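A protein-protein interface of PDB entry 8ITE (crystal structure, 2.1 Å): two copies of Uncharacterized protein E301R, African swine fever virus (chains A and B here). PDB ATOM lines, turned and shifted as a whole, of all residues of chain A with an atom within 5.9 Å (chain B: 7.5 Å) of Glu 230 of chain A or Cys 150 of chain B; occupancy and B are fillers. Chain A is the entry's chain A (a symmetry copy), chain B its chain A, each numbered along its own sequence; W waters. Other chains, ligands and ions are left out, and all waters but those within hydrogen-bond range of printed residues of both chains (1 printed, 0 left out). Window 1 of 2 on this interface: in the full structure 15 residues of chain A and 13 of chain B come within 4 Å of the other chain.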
ATOM      1  N   PHE A 186      -0.206  21.834  -2.277  1.00  0.00           N
ATOM      2  CA  PHE A 186       0.312  20.670  -2.970  1.00  0.00           C
ATOM      3  C   PHE A 186      -0.342  20.595  -4.343  1.00  0.00           C
ATOM      4  O   PHE A 186      -1.481  21.047  -4.529  1.00  0.00           O
ATOM      5  CB  PHE A 186       0.012  19.389  -2.182  1.00  0.00           C
ATOM      6  CG  PHE A 186       1.041  19.052  -1.138  1.00  0.00           C
ATOM      7  CD1 PHE A 186       2.265  19.706  -1.110  1.00  0.00           C
ATOM      8  CD2 PHE A 186       0.796  18.067  -0.196  1.00  0.00           C
ATOM      9  CE1 PHE A 186       3.220  19.385  -0.156  1.00  0.00           C
ATOM     10  CE2 PHE A 186       1.750  17.738   0.757  1.00  0.00           C
ATOM     11  CZ  PHE A 186       2.963  18.404   0.773  1.00  0.00           C
ATOM     12  N   LYS A 193       2.024  11.406  -4.313  1.00  0.00           N
ATOM     13  CA  LYS A 193       3.321  10.785  -4.077  1.00  0.00           C
ATOM     14  C   LYS A 193       3.591  10.654  -2.581  1.00  0.00           C
ATOM     15  O   LYS A 193       3.953   9.575  -2.098  1.00  0.00           O
ATOM     16  CB  LYS A 193       4.424  11.591  -4.756  1.00  0.00           C
ATOM     17  CG  LYS A 193       5.690  10.784  -4.997  1.00  0.00           C
ATOM     18  CD  LYS A 193       6.827  11.676  -5.432  1.00  0.00           C
ATOM     19  CE  LYS A 193       8.095  10.858  -5.604  1.00  0.00           C
ATOM     20  NZ  LYS A 193       7.923   9.796  -6.644  1.00  0.00           N
ATOM     21  N   THR A 194       3.407  11.746  -1.832  1.00  0.00           N
ATOM     22  CA  THR A 194       3.555  11.693  -0.378  1.00  0.00           C
ATOM     23  C   THR A 194       2.777  10.517   0.207  1.00  0.00           C
ATOM     24  O   THR A 194       3.348   9.625   0.846  1.00  0.00           O
ATOM     25  CB  THR A 194       3.080  13.004   0.261  1.00  0.00           C
ATOM     26  OG1 THR A 194       3.975  14.084  -0.062  1.00  0.00           O
ATOM     27  CG2 THR A 194       2.975  12.842   1.791  1.00  0.00           C
ATOM     28  N   PHE A 195       1.485  10.474  -0.066  1.00  0.00           N
ATOM     29  CA  PHE A 195       0.664   9.430   0.513  1.00  0.00           C
ATOM     30  C   PHE A 195       0.516   8.229  -0.394  1.00  0.00           C
ATOM     31  O   PHE A 195      -0.583   7.893  -0.795  1.00  0.00           O
ATOM     32  CB  PHE A 195      -0.674  10.032   0.921  1.00  0.00           C
ATOM     33  CG  PHE A 195      -0.546  11.110   1.949  1.00  0.00           C
ATOM     34  CD1 PHE A 195      -0.194  10.798   3.245  1.00  0.00           C
ATOM     35  CD2 PHE A 195      -0.747  12.433   1.616  1.00  0.00           C
ATOM     36  CE1 PHE A 195      -0.061  11.782   4.198  1.00  0.00           C
ATOM     37  CE2 PHE A 195      -0.610  13.425   2.562  1.00  0.00           C
ATOM     38  CZ  PHE A 195      -0.270  13.099   3.856  1.00  0.00           C
ATOM     39  N   LEU A 216       8.575  22.533   7.339  1.00  0.00           N
ATOM     40  CA  LEU A 216       7.345  21.762   7.555  1.00  0.00           C
ATOM     41  C   LEU A 216       7.685  20.293   7.609  1.00  0.00           C
ATOM     42  O   LEU A 216       8.326  19.771   6.727  1.00  0.00           O
ATOM     43  CB  LEU A 216       6.308  22.019   6.470  1.00  0.00           C
ATOM     44  CG  LEU A 216       5.046  21.157   6.460  1.00  0.00           C
ATOM     45  CD1 LEU A 216       4.059  21.639   7.505  1.00  0.00           C
ATOM     46  CD2 LEU A 216       4.409  21.133   5.084  1.00  0.00           C
ATOM     47  N   HIS A 217       7.261  19.636   8.665  1.00  0.00           N
ATOM     48  CA  HIS A 217       7.561  18.241   8.817  1.00  0.00           C
ATOM     49  C   HIS A 217       6.332  17.385   8.726  1.00  0.00           C
ATOM     50  O   HIS A 217       5.323  17.684   9.325  1.00  0.00           O
ATOM     51  CB  HIS A 217       8.225  17.936  10.158  1.00  0.00           C
ATOM     52  CG  HIS A 217       9.328  18.854  10.561  1.00  0.00           C
ATOM     53  ND1 HIS A 217       9.128  19.931  11.395  1.00  0.00           N
ATOM     54  CD2 HIS A 217      10.658  18.797  10.333  1.00  0.00           C
ATOM     55  CE1 HIS A 217      10.284  20.526  11.624  1.00  0.00           C
ATOM     56  NE2 HIS A 217      11.228  19.861  10.985  1.00  0.00           N
ATOM     57  N   LEU A 218       6.437  16.301   7.997  1.00  0.00           N
ATOM     58  CA  LEU A 218       5.346  15.384   7.864  1.00  0.00           C
ATOM     59  C   LEU A 218       5.911  14.025   8.182  1.00  0.00           C
ATOM     60  O   LEU A 218       6.886  13.623   7.583  1.00  0.00           O
ATOM     61  CB  LEU A 218       4.834  15.394   6.437  1.00  0.00           C
ATOM     62  CG  LEU A 218       3.512  16.013   6.005  1.00  0.00           C
ATOM     63  CD1 LEU A 218       3.390  17.457   6.444  1.00  0.00           C
ATOM     64  CD2 LEU A 218       3.415  15.921   4.494  1.00  0.00           C
ATOM     65  N   TYR A 219       5.321  13.321   9.133  1.00  0.00           N
ATOM     66  CA  TYR A 219       5.765  11.974   9.411  1.00  0.00           C
ATOM     67  C   TYR A 219       4.752  10.891   9.610  1.00  0.00           C
ATOM     68  O   TYR A 219       3.787  11.081  10.295  1.00  0.00           O
ATOM     69  CB  TYR A 219       6.866  11.881  10.465  1.00  0.00           C
ATOM     70  CG  TYR A 219       6.674  12.391  11.859  1.00  0.00           C
ATOM     71  CD1 TYR A 219       6.566  11.504  12.911  1.00  0.00           C
ATOM     72  CD2 TYR A 219       6.737  13.739  12.146  1.00  0.00           C
ATOM     73  CE1 TYR A 219       6.449  11.946  14.211  1.00  0.00           C
ATOM     74  CE2 TYR A 219       6.620  14.192  13.442  1.00  0.00           C
ATOM     75  CZ  TYR A 219       6.470  13.289  14.470  1.00  0.00           C
ATOM     76  OH  TYR A 219       6.345  13.726  15.763  1.00  0.00           O
ATOM     77  N   PHE A 220       5.010   9.744   9.008  1.00  0.00           N
ATOM     78  CA  PHE A 220       4.116   8.618   9.105  1.00  0.00           C
ATOM     79  C   PHE A 220       4.842   7.316   8.914  1.00  0.00           C
ATOM     80  O   PHE A 220       6.036   7.302   8.714  1.00  0.00           O
ATOM     81  CB  PHE A 220       2.966   8.676   8.100  1.00  0.00           C
ATOM     82  CG  PHE A 220       3.336   9.100   6.705  1.00  0.00           C
ATOM     83  CD1 PHE A 220       3.482  10.437   6.373  1.00  0.00           C
ATOM     84  CD2 PHE A 220       3.418   8.164   5.698  1.00  0.00           C
ATOM     85  CE1 PHE A 220       3.780  10.821   5.090  1.00  0.00           C
ATOM     86  CE2 PHE A 220       3.705   8.543   4.407  1.00  0.00           C
ATOM     87  CZ  PHE A 220       3.885   9.872   4.104  1.00  0.00           C
ATOM     88  N   LYS A 222       5.403   4.162   6.545  1.00  0.00           N
ATOM     89  CA  LYS A 222       5.204   3.677   5.195  1.00  0.00           C
ATOM     90  C   LYS A 222       5.235   2.174   5.211  1.00  0.00           C
ATOM     91  O   LYS A 222       5.157   1.571   6.274  1.00  0.00           O
ATOM     92  CB  LYS A 222       6.276   4.211   4.252  1.00  0.00           C
ATOM     93  CG  LYS A 222       5.875   5.499   3.561  1.00  0.00           C
ATOM     94  CD  LYS A 222       6.525   5.653   2.201  1.00  0.00           C
ATOM     95  CE  LYS A 222       5.828   6.736   1.397  1.00  0.00           C
ATOM     96  NZ  LYS A 222       6.485   6.998   0.090  1.00  0.00           N
ATOM     97  N   TYR A 228       8.861   7.115   8.191  1.00  0.00           N
ATOM     98  CA  TYR A 228       9.154   7.927   7.026  1.00  0.00           C
ATOM     99  C   TYR A 228       8.884   9.380   7.390  1.00  0.00           C
ATOM    100  O   TYR A 228       7.968   9.668   8.167  1.00  0.00           O
ATOM    101  CB  TYR A 228       8.312   7.448   5.837  1.00  0.00           C
ATOM    102  CG  TYR A 228       8.409   8.324   4.619  1.00  0.00           C
ATOM    103  CD1 TYR A 228       9.518   8.264   3.772  1.00  0.00           C
ATOM    104  CD2 TYR A 228       7.380   9.200   4.302  1.00  0.00           C
ATOM    105  CE1 TYR A 228       9.599   9.071   2.663  1.00  0.00           C
ATOM    106  CE2 TYR A 228       7.451  10.005   3.209  1.00  0.00           C
ATOM    107  CZ  TYR A 228       8.561   9.941   2.382  1.00  0.00           C
ATOM    108  OH  TYR A 228       8.610  10.770   1.280  1.00  0.00           O
ATOM    109  N   HIS A 229       9.715  10.290   6.879  1.00  0.00           N
ATOM    110  CA  HIS A 229       9.699  11.690   7.299  1.00  0.00           C
ATOM    111  C   HIS A 229       9.940  12.553   6.064  1.00  0.00           C
ATOM    112  O   HIS A 229      10.922  12.333   5.348  1.00  0.00           O
ATOM    113  CB  HIS A 229      10.780  11.939   8.374  1.00  0.00           C
ATOM    114  CG  HIS A 229      10.463  13.052   9.333  1.00  0.00           C
ATOM    115  ND1 HIS A 229      10.678  14.384   9.032  1.00  0.00           N
ATOM    116  CD2 HIS A 229       9.972  13.032  10.598  1.00  0.00           C
ATOM    117  CE1 HIS A 229      10.306  15.135  10.055  1.00  0.00           C
ATOM    118  NE2 HIS A 229       9.883  14.340  11.024  1.00  0.00           N
ATOM    119  N   GLU A 230       9.047  13.514   5.791  1.00  0.00           N
ATOM    120  CA  GLU A 230       9.274  14.528   4.764  1.00  0.00           C
ATOM    121  C   GLU A 230       9.483  15.872   5.449  1.00  0.00           C
ATOM    122  O   GLU A 230       8.744  16.225   6.369  1.00  0.00           O
ATOM    123  CB  GLU A 230       8.108  14.621   3.768  1.00  0.00           C
ATOM    124  CG  GLU A 230       7.924  13.378   2.902  1.00  0.00           C
ATOM    125  CD  GLU A 230       6.805  13.480   1.845  1.00  0.00           C
ATOM    126  OE1 GLU A 230       6.089  14.494   1.787  1.00  0.00           O
ATOM    127  OE2 GLU A 230       6.659  12.521   1.060  1.00  0.00           O
ATOM    128  N   MET A 231      10.489  16.615   4.998  1.00  0.00           N
ATOM    129  CA  MET A 231      10.859  17.895   5.583  1.00  0.00           C
ATOM    130  C   MET A 231      10.934  18.919   4.462  1.00  0.00           C
ATOM    131  O   MET A 231      11.731  18.758   3.535  1.00  0.00           O
ATOM    132  CB  MET A 231      12.195  17.793   6.319  1.00  0.00           C
ATOM    133  CG  MET A 231      12.425  18.883   7.348  1.00  0.00           C
ATOM    134  SD  MET A 231      14.026  18.739   8.151  1.00  0.00           S
ATOM    135  CE  MET A 231      15.116  19.356   6.858  1.00  0.00           C
ATOM    136  N   TYR A 232      10.116  19.970   4.549  1.00  0.00           N
ATOM    137  CA  TYR A 232      10.004  20.982   3.498  1.00  0.00           C
ATOM    138  C   TYR A 232      10.854  22.177   3.921  1.00  0.00           C
ATOM    139  O   TYR A 232      10.464  22.950   4.791  1.00  0.00           O
ATOM    140  CB  TYR A 232       8.535  21.346   3.266  1.00  0.00           C
ATOM    141  CG  TYR A 232       7.782  20.197   2.640  1.00  0.00           C
ATOM    142  CD1 TYR A 232       7.263  19.161   3.426  1.00  0.00           C
ATOM    143  CD2 TYR A 232       7.640  20.110   1.261  1.00  0.00           C
ATOM    144  CE1 TYR A 232       6.607  18.081   2.841  1.00  0.00           C
ATOM    145  CE2 TYR A 232       6.985  19.044   0.673  1.00  0.00           C
ATOM    146  CZ  TYR A 232       6.464  18.032   1.472  1.00  0.00           C
ATOM    147  OH  TYR A 232       5.817  16.968   0.886  1.00  0.00           O
ATOM    148  N   PHE B 122      15.802  11.690  -8.672  1.00  0.00           N
ATOM    149  CA  PHE B 122      16.614  11.724  -7.459  1.00  0.00           C
ATOM    150  C   PHE B 122      18.027  12.147  -7.818  1.00  0.00           C
ATOM    151  O   PHE B 122      18.704  11.490  -8.615  1.00  0.00           O
ATOM    152  CB  PHE B 122      16.654  10.344  -6.790  1.00  0.00           C
ATOM    153  CG  PHE B 122      15.364   9.928  -6.133  1.00  0.00           C
ATOM    154  CD1 PHE B 122      14.209   9.725  -6.889  1.00  0.00           C
ATOM    155  CD2 PHE B 122      15.316   9.683  -4.768  1.00  0.00           C
ATOM    156  CE1 PHE B 122      13.013   9.316  -6.281  1.00  0.00           C
ATOM    157  CE2 PHE B 122      14.116   9.276  -4.151  1.00  0.00           C
ATOM    158  CZ  PHE B 122      12.971   9.094  -4.915  1.00  0.00           C
ATOM    159  N   THR B 126      21.787   9.996   0.671  1.00  0.00           N
ATOM    160  CA  THR B 126      22.619  10.055   1.863  1.00  0.00           C
ATOM    161  C   THR B 126      22.245   8.907   2.790  1.00  0.00           C
ATOM    162  O   THR B 126      21.064   8.551   2.928  1.00  0.00           O
ATOM    163  CB  THR B 126      22.475  11.416   2.571  1.00  0.00           C
ATOM    164  OG1 THR B 126      22.884  12.442   1.670  1.00  0.00           O
ATOM    165  CG2 THR B 126      23.348  11.511   3.813  1.00  0.00           C
ATOM    166  N   PHE B 139      18.262   6.449   5.516  1.00  0.00           N
ATOM    167  CA  PHE B 139      18.436   6.758   4.099  1.00  0.00           C
ATOM    168  C   PHE B 139      17.721   8.073   3.816  1.00  0.00           C
ATOM    169  O   PHE B 139      16.533   8.203   4.133  1.00  0.00           O
ATOM    170  CB  PHE B 139      17.883   5.641   3.211  1.00  0.00           C
ATOM    171  CG  PHE B 139      18.658   4.354   3.284  1.00  0.00           C
ATOM    172  CD1 PHE B 139      18.415   3.439   4.296  1.00  0.00           C
ATOM    173  CD2 PHE B 139      19.630   4.056   2.327  1.00  0.00           C
ATOM    174  CE1 PHE B 139      19.118   2.262   4.359  1.00  0.00           C
ATOM    175  CE2 PHE B 139      20.343   2.881   2.382  1.00  0.00           C
ATOM    176  CZ  PHE B 139      20.102   1.976   3.381  1.00  0.00           C
ATOM    177  N   ILE B 140      18.423   9.036   3.204  1.00  0.00           N
ATOM    178  CA  ILE B 140      17.860  10.362   2.931  1.00  0.00           C
ATOM    179  C   ILE B 140      17.928  10.665   1.444  1.00  0.00           C
ATOM    180  O   ILE B 140      19.017  10.703   0.860  1.00  0.00           O
ATOM    181  CB  ILE B 140      18.562  11.477   3.724  1.00  0.00           C
ATOM    182  CG1 ILE B 140      18.453  11.238   5.226  1.00  0.00           C
ATOM    183  CG2 ILE B 140      17.923  12.842   3.392  1.00  0.00           C
ATOM    184  CD1 ILE B 140      19.772  11.097   5.936  1.00  0.00           C
ATOM    185  N   PHE B 141      16.780  10.963   0.846  1.00  0.00           N
ATOM    186  CA  PHE B 141      16.707  11.369  -0.550  1.00  0.00           C
ATOM    187  C   PHE B 141      16.195  12.805  -0.635  1.00  0.00           C
ATOM    188  O   PHE B 141      15.139  13.115  -0.078  1.00  0.00           O
ATOM    189  CB  PHE B 141      15.785  10.413  -1.307  1.00  0.00           C
ATOM    190  CG  PHE B 141      16.148   8.946  -1.126  1.00  0.00           C
ATOM    191  CD1 PHE B 141      17.071   8.338  -1.969  1.00  0.00           C
ATOM    192  CD2 PHE B 141      15.566   8.186  -0.123  1.00  0.00           C
ATOM    193  CE1 PHE B 141      17.398   6.993  -1.820  1.00  0.00           C
ATOM    194  CE2 PHE B 141      15.894   6.840   0.037  1.00  0.00           C
ATOM    195  CZ  PHE B 141      16.808   6.246  -0.819  1.00  0.00           C
ATOM    196  N   THR B 142      16.924  13.684  -1.328  1.00  0.00           N
ATOM    197  CA  THR B 142      16.501  15.079  -1.465  1.00  0.00           C
ATOM    198  C   THR B 142      15.968  15.357  -2.868  1.00  0.00           C
ATOM    199  O   THR B 142      16.599  14.978  -3.864  1.00  0.00           O
ATOM    200  CB  THR B 142      17.643  16.050  -1.130  1.00  0.00           C
ATOM    201  OG1 THR B 142      18.059  15.851   0.228  1.00  0.00           O
ATOM    202  CG2 THR B 142      17.188  17.513  -1.299  1.00  0.00           C
ATOM    203  N   ASP B 143      14.800  16.014  -2.928  1.00  0.00           N
ATOM    204  CA  ASP B 143      14.199  16.543  -4.156  1.00  0.00           C
ATOM    205  C   ASP B 143      14.470  18.044  -4.191  1.00  0.00           C
ATOM    206  O   ASP B 143      13.934  18.805  -3.376  1.00  0.00           O
ATOM    207  CB  ASP B 143      12.697  16.227  -4.205  1.00  0.00           C
ATOM    208  CG  ASP B 143      11.869  17.212  -5.074  1.00  0.00           C
ATOM    209  OD1 ASP B 143      12.410  17.934  -5.944  1.00  0.00           O
ATOM    210  OD2 ASP B 143      10.628  17.228  -4.908  1.00  0.00           O
ATOM    211  N   ILE B 146      11.733  21.342  -4.975  1.00  0.00           N
ATOM    212  CA  ILE B 146      11.011  22.035  -3.919  1.00  0.00           C
ATOM    213  C   ILE B 146      11.744  22.019  -2.593  1.00  0.00           C
ATOM    214  O   ILE B 146      11.233  22.577  -1.616  1.00  0.00           O
ATOM    215  CB  ILE B 146       9.582  21.479  -3.754  1.00  0.00           C
ATOM    216  CG1 ILE B 146       9.596  19.953  -3.638  1.00  0.00           C
ATOM    217  CG2 ILE B 146       8.717  21.909  -4.933  1.00  0.00           C
ATOM    218  CD1 ILE B 146       8.224  19.381  -3.286  1.00  0.00           C
ATOM    219  N   ASP B 147      12.948  21.435  -2.541  1.00  0.00           N
ATOM    220  CA  ASP B 147      13.769  21.374  -1.328  1.00  0.00           C
ATOM    221  C   ASP B 147      13.078  20.583  -0.215  1.00  0.00           C
ATOM    222  O   ASP B 147      12.980  21.031   0.931  1.00  0.00           O
ATOM    223  CB  ASP B 147      14.159  22.772  -0.832  1.00  0.00           C
ATOM    224  CG  ASP B 147      15.156  23.471  -1.750  1.00  0.00           C
ATOM    225  OD1 ASP B 147      15.955  22.785  -2.440  1.00  0.00           O
ATOM    226  OD2 ASP B 147      15.123  24.721  -1.784  1.00  0.00           O
ATOM    227  N   LYS B 148      12.623  19.378  -0.544  1.00  0.00           N
ATOM    228  CA  LYS B 148      12.101  18.468   0.469  1.00  0.00           C
ATOM    229  C   LYS B 148      13.061  17.290   0.642  1.00  0.00           C
ATOM    230  O   LYS B 148      13.480  16.667  -0.341  1.00  0.00           O
ATOM    231  CB  LYS B 148      10.675  17.998   0.124  1.00  0.00           C
ATOM    232  CG  LYS B 148      10.533  16.757  -0.757  1.00  0.00           C
ATOM    233  CD  LYS B 148       9.057  16.292  -0.865  1.00  0.00           C
ATOM    234  CE  LYS B 148       8.877  15.175  -1.888  1.00  0.00           C
ATOM    235  NZ  LYS B 148       7.444  14.689  -1.944  1.00  0.00           N
ATOM    236  N   GLU B 149      13.401  17.013   1.889  1.00  0.00           N
ATOM    237  CA  GLU B 149      14.231  15.871   2.205  1.00  0.00           C
ATOM    238  C   GLU B 149      13.314  14.772   2.699  1.00  0.00           C
ATOM    239  O   GLU B 149      12.518  14.995   3.588  1.00  0.00           O
ATOM    240  CB  GLU B 149      15.225  16.221   3.302  1.00  0.00           C
ATOM    241  CG  GLU B 149      16.352  17.127   2.883  1.00  0.00           C
ATOM    242  CD  GLU B 149      17.438  17.182   3.929  1.00  0.00           C
ATOM    243  OE1 GLU B 149      17.271  16.541   4.984  1.00  0.00           O
ATOM    244  OE2 GLU B 149      18.453  17.865   3.698  1.00  0.00           O
ATOM    245  N   CYS B 150      13.418  13.596   2.112  1.00  0.00           N
ATOM    246  CA  CYS B 150      12.612  12.463   2.511  1.00  0.00           C
ATOM    247  C   CYS B 150      13.477  11.411   3.175  1.00  0.00           C
ATOM    248  O   CYS B 150      14.420  10.936   2.579  1.00  0.00           O
ATOM    249  CB  CYS B 150      11.904  11.892   1.287  1.00  0.00           C
ATOM    250  SG  CYS B 150      10.960  13.080   0.326  1.00  0.00           S
ATOM    251  N   THR B 151      13.154  11.032   4.398  1.00  0.00           N
ATOM    252  CA  THR B 151      13.978  10.085   5.147  1.00  0.00           C
ATOM    253  C   THR B 151      13.335   8.762   5.555  1.00  0.00           C
ATOM    254  O   THR B 151      12.220   8.751   6.047  1.00  0.00           O
ATOM    255  CB  THR B 151      14.582  10.769   6.393  1.00  0.00           C
ATOM    256  OG1 THR B 151      15.305  11.930   5.989  1.00  0.00           O
ATOM    257  CG2 THR B 151      15.501   9.845   7.177  1.00  0.00           C
ATOM    258  N   TYR B 152      14.021   7.654   5.324  1.00  0.00           N
ATOM    259  CA  TYR B 152      13.553   6.350   5.773  1.00  0.00           C
ATOM    260  C   TYR B 152      14.425   5.859   6.924  1.00  0.00           C
ATOM    261  O   TYR B 152      15.663   5.927   6.853  1.00  0.00           O
ATOM    262  CB  TYR B 152      13.581   5.335   4.632  1.00  0.00           C
ATOM    263  CG  TYR B 152      12.676   5.616   3.446  1.00  0.00           C
ATOM    264  CD1 TYR B 152      12.992   6.603   2.512  1.00  0.00           C
ATOM    265  CD2 TYR B 152      11.545   4.836   3.218  1.00  0.00           C
ATOM    266  CE1 TYR B 152      12.182   6.833   1.408  1.00  0.00           C
ATOM    267  CE2 TYR B 152      10.726   5.058   2.128  1.00  0.00           C
ATOM    268  CZ  TYR B 152      11.046   6.047   1.226  1.00  0.00           C
ATOM    269  OH  TYR B 152      10.232   6.245   0.138  1.00  0.00           O
HETATM  270  O   HOH W   1      13.425  14.032   5.902  1.00  0.00           O
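No position is printed for both chains.
Of the printed residues of chain B, Glu 230 of chain A touches Lys 148, Glu 149 and Cys 150.
Of the printed residues of chain A, Tyr 152 of chain B touches Lys 222 and Tyr 228.
Printed residues of chain A within 4 Å of Lys 148 of chain B: Thr 194 (3.99 Å), Glu 230 (3.8 Å), Met 231 (3.1 Å) and Tyr 232 (3.7 Å).
The nearest printed residue of chain B that does not touch Tyr 232 of chain A is Ile 146 of chain B (4.2 Å).
The backbone NH (N) of Glu 149 of chain B sits at hydrogen-bond distance from the backbone carbonyl oxygen (O) of Met 231 of chain A (2.9 Å).
SG of Cys 150 of chain B sits at hydrogen-bond distance from OH of Tyr 228 of chain A.
The backbone NH of Thr 151 of chain B lies within hydrogen-bond range of the backbone carbonyl oxygen of His 229 of chain A (2.8 Å).
The side-chain carboxylate of Glu 230 of chain A is in salt-bridge range of the side-chain amino group of Lys 148 of chain B (3.8 Å).
Water W1 lies within hydrogen-bond range of the backbone carbonyl oxygen of Glu 149 of chain B, the side-chain hydroxyl of Thr 151 of chain B and the backbone carbonyl oxygen of His 229 of chain A.
Of the 14 printed residues of chain B, 6 touch a printed residue of chain A.
Of the 15 printed residues of chain A, 7 touch a printed residue of chain B.
Hydrophobic or aromatic side chains of chain A within 4 Å of the printed part of chain B: Tyr 228, Met 231 and Tyr 232.
Among the printed residues, 16 pairs touch across the chains.
Among the printed residues, Asp or Glu carboxylates within 4 Å of a Lys or Arg side-chain nitrogen of the other chain: Glu 230 of chain A with Lys 148 of chain B (3.8 Å).
OE1 of Glu 230 of chain A sits at hydrogen-bond distance from OH of Tyr 232 of chain A, at 2.6 Å.
The backbone carbonyl oxygen (O) of Leu 218 of chain A is in hydrogen-bond range of the backbone NH (N) of Glu 230 of chain A (2.8 Å).
The backbone NH (N) of Tyr 232 of chain A lies within hydrogen-bond range of the backbone carbonyl oxygen (O) of Leu 216 of chain A, 2.8 Å away.
O of Lys 148 of chain B lies within hydrogen-bond range of N of Asp 143 of chain B (3.0 Å).
The backbone carbonyl oxygen of Phe 139 of chain B sits at hydrogen-bond distance from the backbone NH of Tyr 152 of chain B, at 2.8 Å.
The backbone carbonyl oxygen (O) of Phe 141 of chain B is in hydrogen-bond range of the backbone NH (N) of Cys 150 of chain B, at 2.8 Å.
OG1 of Thr 194 of chain A touches NZ of Lys 148 of chain B, at 3.99 Å.
NZ of Lys 222 of chain A touches OH of Tyr 152 of chain B, 3.8 Å away.
Tyr 228 of chain A touches Thr 151 of chain B (CA to O, 3.3 Å).
O of His 229 of chain A touches O of Glu 149 of chain B, 3.6 Å away.
His 229 of chain A touches Cys 150 of chain B.
Glu 149 of chain B touches Glu 230 of chain A.
Cys 150 of chain B touches Glu 230 of chain A (SG to CG, 3.99 Å).
Asp 147 of chain B touches Met 231 of chain A (O to O, 3.7 Å).
Met 231 of chain A touches Lys 148 of chain B.
CD of Lys 148 of chain B touches OH of Tyr 232 of chain A (3.7 Å).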
